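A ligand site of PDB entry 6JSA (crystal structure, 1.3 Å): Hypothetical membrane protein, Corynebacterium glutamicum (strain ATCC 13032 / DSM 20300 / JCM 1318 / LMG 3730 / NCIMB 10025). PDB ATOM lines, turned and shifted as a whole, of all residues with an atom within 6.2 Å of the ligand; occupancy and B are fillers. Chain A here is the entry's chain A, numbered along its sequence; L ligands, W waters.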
ATOM      1  N   LYS A  15     -11.868  21.678  -3.983  1.00  0.00           N
ATOM      2  CA  LYS A  15     -12.045  20.459  -4.771  1.00  0.00           C
ATOM      3  C   LYS A  15     -10.959  20.443  -5.834  1.00  0.00           C
ATOM      4  O   LYS A  15     -10.799  21.440  -6.558  1.00  0.00           O
ATOM      5  CB  LYS A  15     -13.426  20.408  -5.426  1.00  0.00           C
ATOM      6  CG  LYS A  15     -13.779  19.044  -6.017  1.00  0.00           C
ATOM      7  CD  LYS A  15     -15.198  19.059  -6.572  1.00  0.00           C
ATOM      8  CE  LYS A  15     -15.708  17.684  -7.019  1.00  0.00           C
ATOM      9  NZ  LYS A  15     -14.734  16.825  -7.735  1.00  0.00           N
ATOM     10  N   ALA A  16     -10.209  19.339  -5.931  1.00  0.00           N
ATOM     11  CA  ALA A  16      -9.088  19.319  -6.873  1.00  0.00           C
ATOM     12  C   ALA A  16      -9.554  19.576  -8.304  1.00  0.00           C
ATOM     13  O   ALA A  16      -8.922  20.340  -9.044  1.00  0.00           O
ATOM     14  CB  ALA A  16      -8.349  17.980  -6.794  1.00  0.00           C
ATOM     15  N   SER A  17     -10.667  18.958  -8.714  1.00  0.00           N
ATOM     16  CA  SER A  17     -11.135  19.165 -10.070  1.00  0.00           C
ATOM     17  C   SER A  17     -11.577  20.614 -10.298  1.00  0.00           C
ATOM     18  O   SER A  17     -11.480  21.116 -11.418  1.00  0.00           O
ATOM     19  CB  SER A  17     -12.239  18.163 -10.427  1.00  0.00           C
ATOM     20  OG  SER A  17     -13.397  18.363  -9.641  1.00  0.00           O
ATOM     21  N   PHE A  18     -12.062  21.282  -9.252  1.00  0.00           N
ATOM     22  CA  PHE A  18     -12.384  22.703  -9.378  1.00  0.00           C
ATOM     23  C   PHE A  18     -11.132  23.542  -9.591  1.00  0.00           C
ATOM     24  O   PHE A  18     -11.124  24.440 -10.437  1.00  0.00           O
ATOM     25  CB  PHE A  18     -13.163  23.187  -8.147  1.00  0.00           C
ATOM     26  CG  PHE A  18     -13.660  24.597  -8.275  1.00  0.00           C
ATOM     27  CD1 PHE A  18     -14.607  24.920  -9.232  1.00  0.00           C
ATOM     28  CD2 PHE A  18     -13.195  25.593  -7.438  1.00  0.00           C
ATOM     29  CE1 PHE A  18     -15.095  26.206  -9.362  1.00  0.00           C
ATOM     30  CE2 PHE A  18     -13.668  26.901  -7.548  1.00  0.00           C
ATOM     31  CZ  PHE A  18     -14.624  27.205  -8.517  1.00  0.00           C
ATOM     32  N   GLN A  19     -10.063  23.265  -8.830  1.00  0.00           N
ATOM     33  CA  GLN A  19      -8.801  23.961  -9.066  1.00  0.00           C
ATOM     34  C   GLN A  19      -8.346  23.796 -10.513  1.00  0.00           C
ATOM     35  O   GLN A  19      -7.933  24.760 -11.163  1.00  0.00           O
ATOM     36  CB  GLN A  19      -7.703  23.402  -8.171  1.00  0.00           C
ATOM     37  CG  GLN A  19      -7.800  23.754  -6.708  1.00  0.00           C
ATOM     38  CD  GLN A  19      -6.678  23.094  -5.930  1.00  0.00           C
ATOM     39  OE1 GLN A  19      -5.594  22.869  -6.460  1.00  0.00           O
ATOM     40  NE2 GLN A  19      -6.939  22.767  -4.674  1.00  0.00           N
ATOM     41  N   TYR A  21     -10.073  23.000 -13.145  1.00  0.00           N
ATOM     42  CA  TYR A  21     -10.975  23.731 -14.021  1.00  0.00           C
ATOM     43  C   TYR A  21     -10.664  25.223 -14.018  1.00  0.00           C
ATOM     44  O   TYR A  21     -10.535  25.848 -15.075  1.00  0.00           O
ATOM     45  CB  TYR A  21     -12.419  23.458 -13.579  1.00  0.00           C
ATOM     46  CG  TYR A  21     -13.427  24.455 -14.092  1.00  0.00           C
ATOM     47  CD1 TYR A  21     -13.741  24.516 -15.439  1.00  0.00           C
ATOM     48  CD2 TYR A  21     -14.064  25.324 -13.210  1.00  0.00           C
ATOM     49  CE1 TYR A  21     -14.670  25.420 -15.901  1.00  0.00           C
ATOM     50  CE2 TYR A  21     -14.992  26.224 -13.658  1.00  0.00           C
ATOM     51  CZ  TYR A  21     -15.287  26.274 -15.004  1.00  0.00           C
ATOM     52  OH  TYR A  21     -16.197  27.177 -15.454  1.00  0.00           O
ATOM     53  N   ILE A  26     -10.667  26.202 -20.161  1.00  0.00           N
ATOM     54  CA  ILE A  26     -12.074  26.560 -20.329  1.00  0.00           C
ATOM     55  C   ILE A  26     -12.389  27.796 -19.484  1.00  0.00           C
ATOM     56  O   ILE A  26     -12.853  28.814 -19.989  1.00  0.00           O
ATOM     57  CB  ILE A  26     -13.002  25.377 -20.012  1.00  0.00           C
ATOM     58  CG1 ILE A  26     -12.805  24.279 -21.068  1.00  0.00           C
ATOM     59  CG2 ILE A  26     -14.447  25.850 -19.923  1.00  0.00           C
ATOM     60  CD1 ILE A  26     -13.494  22.964 -20.749  1.00  0.00           C
ATOM     61  N   HIS A  72     -13.675  32.995 -16.639  1.00  0.00           N
ATOM     62  CA  HIS A  72     -14.626  33.409 -17.680  1.00  0.00           C
ATOM     63  C   HIS A  72     -14.744  34.937 -17.756  1.00  0.00           C
ATOM     64  O   HIS A  72     -15.842  35.499 -17.755  1.00  0.00           O
ATOM     65  CB  HIS A  72     -15.992  32.764 -17.459  1.00  0.00           C
ATOM     66  CG  HIS A  72     -15.962  31.265 -17.548  1.00  0.00           C
ATOM     67  ND1 HIS A  72     -15.891  30.596 -18.754  1.00  0.00           N
ATOM     68  CD2 HIS A  72     -15.981  30.317 -16.583  1.00  0.00           C
ATOM     69  CE1 HIS A  72     -15.892  29.299 -18.531  1.00  0.00           C
ATOM     70  NE2 HIS A  72     -15.945  29.096 -17.221  1.00  0.00           N
ATOM     71  N   ILE A  75     -16.961  36.550 -15.089  1.00  0.00           N
ATOM     72  CA  ILE A  75     -18.294  36.008 -14.827  1.00  0.00           C
ATOM     73  C   ILE A  75     -18.266  35.096 -13.603  1.00  0.00           C
ATOM     74  O   ILE A  75     -19.133  35.178 -12.729  1.00  0.00           O
ATOM     75  CB  ILE A  75     -18.851  35.290 -16.066  1.00  0.00           C
ATOM     76  CG1 ILE A  75     -19.172  36.300 -17.168  1.00  0.00           C
ATOM     77  CG2 ILE A  75     -20.084  34.489 -15.695  1.00  0.00           C
ATOM     78  CD1 ILE A  75     -20.375  37.158 -16.868  1.00  0.00           C
ATOM     79  N   LEU A  76     -17.275  34.210 -13.547  1.00  0.00           N
ATOM     80  CA  LEU A  76     -17.038  33.402 -12.357  1.00  0.00           C
ATOM     81  C   LEU A  76     -16.264  34.249 -11.354  1.00  0.00           C
ATOM     82  O   LEU A  76     -15.190  34.771 -11.654  1.00  0.00           O
ATOM     83  CB  LEU A  76     -16.255  32.138 -12.716  1.00  0.00           C
ATOM     84  CG  LEU A  76     -16.168  31.022 -11.667  1.00  0.00           C
ATOM     85  CD1 LEU A  76     -15.828  29.689 -12.336  1.00  0.00           C
ATOM     86  CD2 LEU A  76     -15.134  31.337 -10.586  1.00  0.00           C
ATOM     87  N   ASP A  77     -16.829  34.383 -10.154  1.00  0.00           N
ATOM     88  CA  ASP A  77     -16.270  35.235  -9.113  1.00  0.00           C
ATOM     89  C   ASP A  77     -16.782  34.648  -7.799  1.00  0.00           C
ATOM     90  O   ASP A  77     -17.938  34.869  -7.424  1.00  0.00           O
ATOM     91  CB  ASP A  77     -16.755  36.666  -9.326  1.00  0.00           C
ATOM     92  CG  ASP A  77     -16.127  37.667  -8.368  1.00  0.00           C
ATOM     93  OD1 ASP A  77     -15.667  37.270  -7.269  1.00  0.00           O
ATOM     94  OD2 ASP A  77     -16.119  38.859  -8.706  1.00  0.00           O
ATOM     95  N   MET A  78     -15.922  33.878  -7.130  1.00  0.00           N
ATOM     96  CA  MET A  78     -16.322  33.111  -5.960  1.00  0.00           C
ATOM     97  C   MET A  78     -15.352  33.403  -4.832  1.00  0.00           C
ATOM     98  O   MET A  78     -14.143  33.161  -4.975  1.00  0.00           O
ATOM     99  CB  MET A  78     -16.352  31.614  -6.256  1.00  0.00           C
ATOM    100  CG  MET A  78     -16.843  30.786  -5.085  1.00  0.00           C
ATOM    101  SD  MET A  78     -16.880  29.031  -5.482  1.00  0.00           S
ATOM    102  CE  MET A  78     -17.978  28.413  -4.215  1.00  0.00           C
ATOM    103  N   SER A 100     -20.728  34.487  -4.348  1.00  0.00           N
ATOM    104  CA  SER A 100     -20.438  33.845  -5.620  1.00  0.00           C
ATOM    105  C   SER A 100     -21.393  34.341  -6.688  1.00  0.00           C
ATOM    106  O   SER A 100     -22.505  34.788  -6.392  1.00  0.00           O
ATOM    107  CB  SER A 100     -20.542  32.324  -5.526  1.00  0.00           C
ATOM    108  OG  SER A 100     -19.854  31.699  -6.579  1.00  0.00           O
ATOM    109  N   SER A 101     -20.961  34.234  -7.950  1.00  0.00           N
ATOM    110  CA  SER A 101     -21.761  34.638  -9.097  1.00  0.00           C
ATOM    111  C   SER A 101     -22.274  33.433  -9.872  1.00  0.00           C
ATOM    112  O   SER A 101     -21.648  32.367  -9.895  1.00  0.00           O
ATOM    113  CB  SER A 101     -20.937  35.519 -10.037  1.00  0.00           C
ATOM    114  OG  SER A 101     -20.741  36.796  -9.472  1.00  0.00           O
ATOM    115  N   ASP A 102     -23.428  33.608 -10.526  1.00  0.00           N
ATOM    116  CA  ASP A 102     -23.972  32.616 -11.448  1.00  0.00           C
ATOM    117  C   ASP A 102     -23.421  32.853 -12.853  1.00  0.00           C
ATOM    118  O   ASP A 102     -22.586  33.723 -13.074  1.00  0.00           O
ATOM    119  CB  ASP A 102     -25.507  32.601 -11.362  1.00  0.00           C
ATOM    120  CG  ASP A 102     -26.145  33.889 -11.866  1.00  0.00           C
ATOM    121  OD1 ASP A 102     -25.483  34.706 -12.557  1.00  0.00           O
ATOM    122  OD2 ASP A 102     -27.341  34.102 -11.563  1.00  0.00           O
ATOM    123  N   MET A 103     -23.902  32.061 -13.819  1.00  0.00           N
ATOM    124  CA  MET A 103     -23.384  32.160 -15.187  1.00  0.00           C
ATOM    125  C   MET A 103     -23.777  33.456 -15.893  1.00  0.00           C
ATOM    126  O   MET A 103     -23.206  33.751 -16.947  1.00  0.00           O
ATOM    127  CB  MET A 103     -23.766  30.942 -16.036  1.00  0.00           C
ATOM    128  CG  MET A 103     -22.688  29.889 -16.043  1.00  0.00           C
ATOM    129  SD  MET A 103     -22.777  28.622 -17.327  1.00  0.00           S
ATOM    130  CE  MET A 103     -22.630  29.580 -18.830  1.00  0.00           C
ATOM    131  N   ASP A 104     -24.732  34.210 -15.368  1.00  0.00           N
ATOM    132  CA  ASP A 104     -25.033  35.553 -15.872  1.00  0.00           C
ATOM    133  C   ASP A 104     -24.144  36.609 -15.253  1.00  0.00           C
ATOM    134  O   ASP A 104     -24.277  37.797 -15.595  1.00  0.00           O
ATOM    135  CB  ASP A 104     -26.502  35.892 -15.634  1.00  0.00           C
ATOM    136  CG  ASP A 104     -27.406  35.365 -16.716  1.00  0.00           C
ATOM    137  OD1 ASP A 104     -27.261  35.801 -17.877  1.00  0.00           O
ATOM    138  OD2 ASP A 104     -28.251  34.490 -16.405  1.00  0.00           O
ATOM    139  N   GLY A 105     -23.252  36.227 -14.351  1.00  0.00           N
ATOM    140  CA  GLY A 105     -22.457  37.191 -13.636  1.00  0.00           C
ATOM    141  C   GLY A 105     -23.167  37.830 -12.464  1.00  0.00           C
ATOM    142  O   GLY A 105     -22.641  38.805 -11.910  1.00  0.00           O
ATOM    143  N   ALA A 145     -23.739  28.121  -4.628  1.00  0.00           N
ATOM    144  CA  ALA A 145     -22.561  28.970  -4.798  1.00  0.00           C
ATOM    145  C   ALA A 145     -21.678  28.474  -5.936  1.00  0.00           C
ATOM    146  O   ALA A 145     -20.985  29.280  -6.567  1.00  0.00           O
ATOM    147  CB  ALA A 145     -21.774  29.046  -3.496  1.00  0.00           C
ATOM    148  N   PHE A 146     -21.686  27.179  -6.203  1.00  0.00           N
ATOM    149  CA  PHE A 146     -20.997  26.633  -7.366  1.00  0.00           C
ATOM    150  C   PHE A 146     -21.850  26.665  -8.627  1.00  0.00           C
ATOM    151  O   PHE A 146     -21.598  25.896  -9.567  1.00  0.00           O
ATOM    152  CB  PHE A 146     -20.492  25.222  -7.083  1.00  0.00           C
ATOM    153  CG  PHE A 146     -19.252  25.165  -6.234  1.00  0.00           C
ATOM    154  CD1 PHE A 146     -18.034  25.556  -6.750  1.00  0.00           C
ATOM    155  CD2 PHE A 146     -19.293  24.668  -4.933  1.00  0.00           C
ATOM    156  CE1 PHE A 146     -16.887  25.477  -5.992  1.00  0.00           C
ATOM    157  CE2 PHE A 146     -18.144  24.585  -4.161  1.00  0.00           C
ATOM    158  CZ  PHE A 146     -16.930  24.994  -4.694  1.00  0.00           C
ATOM    159  N   ALA A 147     -22.866  27.530  -8.656  1.00  0.00           N
ATOM    160  CA  ALA A 147     -23.681  27.751  -9.857  1.00  0.00           C
ATOM    161  C   ALA A 147     -24.379  26.477 -10.322  1.00  0.00           C
ATOM    162  O   ALA A 147     -24.647  26.307 -11.515  1.00  0.00           O
ATOM    163  CB  ALA A 147     -22.892  28.429 -10.988  1.00  0.00           C
ATOM    164  N   PHE A 149     -23.284  23.575 -10.694  1.00  0.00           N
ATOM    165  CA  PHE A 149     -22.479  22.596 -11.417  1.00  0.00           C
ATOM    166  C   PHE A 149     -22.218  21.338 -10.591  1.00  0.00           C
ATOM    167  O   PHE A 149     -21.946  20.284 -11.174  1.00  0.00           O
ATOM    168  CB  PHE A 149     -21.160  23.200 -11.919  1.00  0.00           C
ATOM    169  CG  PHE A 149     -21.303  24.021 -13.163  1.00  0.00           C
ATOM    170  CD1 PHE A 149     -21.571  25.383 -13.098  1.00  0.00           C
ATOM    171  CD2 PHE A 149     -21.177  23.426 -14.413  1.00  0.00           C
ATOM    172  CE1 PHE A 149     -21.695  26.138 -14.252  1.00  0.00           C
ATOM    173  CE2 PHE A 149     -21.314  24.176 -15.582  1.00  0.00           C
ATOM    174  CZ  PHE A 149     -21.573  25.527 -15.507  1.00  0.00           C
ATOM    175  N   TYR A 150     -22.278  21.432  -9.264  1.00  0.00           N
ATOM    176  CA  TYR A 150     -22.245  20.277  -8.384  1.00  0.00           C
ATOM    177  C   TYR A 150     -23.584  20.214  -7.676  1.00  0.00           C
ATOM    178  O   TYR A 150     -24.136  21.244  -7.271  1.00  0.00           O
ATOM    179  CB  TYR A 150     -21.183  20.424  -7.291  1.00  0.00           C
ATOM    180  CG  TYR A 150     -19.764  20.671  -7.730  1.00  0.00           C
ATOM    181  CD1 TYR A 150     -19.182  19.925  -8.746  1.00  0.00           C
ATOM    182  CD2 TYR A 150     -18.986  21.647  -7.113  1.00  0.00           C
ATOM    183  CE1 TYR A 150     -17.868  20.153  -9.146  1.00  0.00           C
ATOM    184  CE2 TYR A 150     -17.684  21.885  -7.494  1.00  0.00           C
ATOM    185  CZ  TYR A 150     -17.125  21.134  -8.516  1.00  0.00           C
ATOM    186  OH  TYR A 150     -15.825  21.385  -8.900  1.00  0.00           O
HETATM  187  C1  LIG L   1     -17.451  23.293 -15.246  1.00  0.00           C
HETATM  188  C2  LIG L   1     -18.659  26.461 -18.684  1.00  0.00           C
HETATM  189  C3  LIG L   1     -19.436  29.827 -15.298  1.00  0.00           C
HETATM  190  C4  LIG L   1     -18.602  26.547 -11.851  1.00  0.00           C
HETATM  191  C5  LIG L   1     -17.675  23.865 -16.480  1.00  0.00           C
HETATM  192  C6  LIG L   1     -17.457  23.229 -17.763  1.00  0.00           C
HETATM  193  C7  LIG L   1     -17.788  24.092 -18.722  1.00  0.00           C
HETATM  194  C8  LIG L   1     -18.245  25.313 -18.063  1.00  0.00           C
HETATM  195  C9  LIG L   1     -17.719  23.874 -20.251  1.00  0.00           C
HETATM  196  C10 LIG L   1     -16.873  21.815 -17.932  1.00  0.00           C
HETATM  197  C11 LIG L   1     -15.370  21.971 -17.709  1.00  0.00           C
HETATM  198  C12 LIG L   1     -14.655  20.646 -17.749  1.00  0.00           C
HETATM  199  O1  LIG L   1     -15.305  19.594 -17.571  1.00  0.00           O
HETATM  200  O2  LIG L   1     -13.410  20.646 -17.956  1.00  0.00           O
HETATM  201  C13 LIG L   1     -18.919  27.668 -18.086  1.00  0.00           C
HETATM  202  C14 LIG L   1     -19.150  28.930 -18.750  1.00  0.00           C
HETATM  203  C15 LIG L   1     -19.378  29.871 -17.813  1.00  0.00           C
HETATM  204  C16 LIG L   1     -19.276  29.214 -16.529  1.00  0.00           C
HETATM  205  C17 LIG L   1     -19.143  29.082 -20.286  1.00  0.00           C
HETATM  206  C18 LIG L   1     -19.675  31.382 -17.952  1.00  0.00           C
HETATM  207  C19 LIG L   1     -19.667  32.085 -19.088  1.00  0.00           C
HETATM  208  C20 LIG L   1     -19.313  29.228 -14.066  1.00  0.00           C
HETATM  209  C21 LIG L   1     -19.604  29.871 -12.794  1.00  0.00           C
HETATM  210  C22 LIG L   1     -19.344  28.980 -11.834  1.00  0.00           C
HETATM  211  C23 LIG L   1     -18.924  27.743 -12.470  1.00  0.00           C
HETATM  212  C24 LIG L   1     -20.070  31.324 -12.614  1.00  0.00           C
HETATM  213  C25 LIG L   1     -19.510  29.242 -10.322  1.00  0.00           C
HETATM  214  C26 LIG L   1     -18.598  28.801  -9.440  1.00  0.00           C
HETATM  215  C27 LIG L   1     -18.240  25.382 -12.480  1.00  0.00           C
HETATM  216  C28 LIG L   1     -17.931  24.151 -11.809  1.00  0.00           C
HETATM  217  C29 LIG L   1     -17.608  23.242 -12.742  1.00  0.00           C
HETATM  218  C30 LIG L   1     -17.697  23.886 -14.032  1.00  0.00           C
HETATM  219  C31 LIG L   1     -17.976  23.937 -10.288  1.00  0.00           C
HETATM  220  C32 LIG L   1     -17.176  21.788 -12.492  1.00  0.00           C
HETATM  221  C33 LIG L   1     -15.646  21.756 -12.450  1.00  0.00           C
HETATM  222  C34 LIG L   1     -15.170  20.375 -12.102  1.00  0.00           C
HETATM  223  O3  LIG L   1     -15.048  19.523 -13.013  1.00  0.00           O
HETATM  224  O4  LIG L   1     -14.916  20.111 -10.898  1.00  0.00           O
HETATM  225  N1  LIG L   1     -18.152  25.142 -16.696  1.00  0.00           N
HETATM  226  N2  LIG L   1     -18.988  27.871 -16.725  1.00  0.00           N
HETATM  227  N3  LIG L   1     -18.907  27.929 -13.825  1.00  0.00           N
HETATM  228  N4  LIG L   1     -18.092  25.200 -13.845  1.00  0.00           N
HETATM  229 FE1  LIG L   1     -18.236  26.634 -15.274  1.00  0.00          FE
HETATM  230  O   HOH W   1     -18.898  32.500  -9.284  1.00  0.00           O
HETATM  231  O   HOH W   2     -11.325  22.398 -17.788  1.00  0.00           O
HETATM  232  O   HOH W   3     -16.635  19.665 -15.273  1.00  0.00           O
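The backbone NH of Ser 101 sits at hydrogen-bond distance from the backbone carbonyl oxygen of Asp 77 (3.1 Å). The backbone carbonyl oxygen of Ala 145 sits at hydrogen-bond distance from the side-chain hydroxyl of Ser 100 (2.7 Å). NZ of Lys 15 lies within hydrogen-bond range of OG of Ser 17 (2.8 Å). The side-chain carboxylate (OD1) of Asp 102 is in hydrogen-bond range of the backbone NH (N) of Asp 104 (3.0 Å). The backbone NH (N) of Gly 105 sits at hydrogen-bond distance from the side-chain carboxylate (OD1) of Asp 102 (3.2 Å). NE2 of His 72 lies close to OH of Tyr 21 (2.6 Å).
A ring nitrogen (NE2) of His 72 lies close to a nitrogen (N2) of the ligand (3.3 Å). Merely in contact with the ligand: Ile 26 (3.6 Å), Ile 75 (3.9 Å), Leu 76 (3.6 Å), Ser 101 (3.3 Å), Asp 102 (3.5 Å), Met 103 (3.3 Å), Ala 145 (3.8 Å), Phe 146 (3.8 Å), Ala 147 (3.5 Å) and Phe 149 (3.3 Å). Hydrophobic or aromatic side chains within 4 Å of the ligand: Phe 18, Tyr 21, Ile 26, His 72, Ile 75, Leu 76, Met 103, Phe 146, Ala 147, Phe 149 and Tyr 150.
An iron atom (FE1) of the ligand is bound by the side-chain hydroxyl (OH) of Tyr 21 (2.1 Å). An oxygen (O4) of the ligand sits at hydrogen-bond distance from the backbone NH of Phe 18 (3.5 Å). The side-chain hydroxyl (OG) of Ser 17 lies within hydrogen-bond range of an oxygen (O4) of the ligand, at 2.6 Å. OH of Tyr 150 lies within hydrogen-bond range of O4 of the ligand (2.5 Å).
Water W1 lies within hydrogen-bond range of O of Ser 101 (2.8 Å), N of Asp 77 (2.9 Å) and OG of Ser 100 (3.0 Å).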
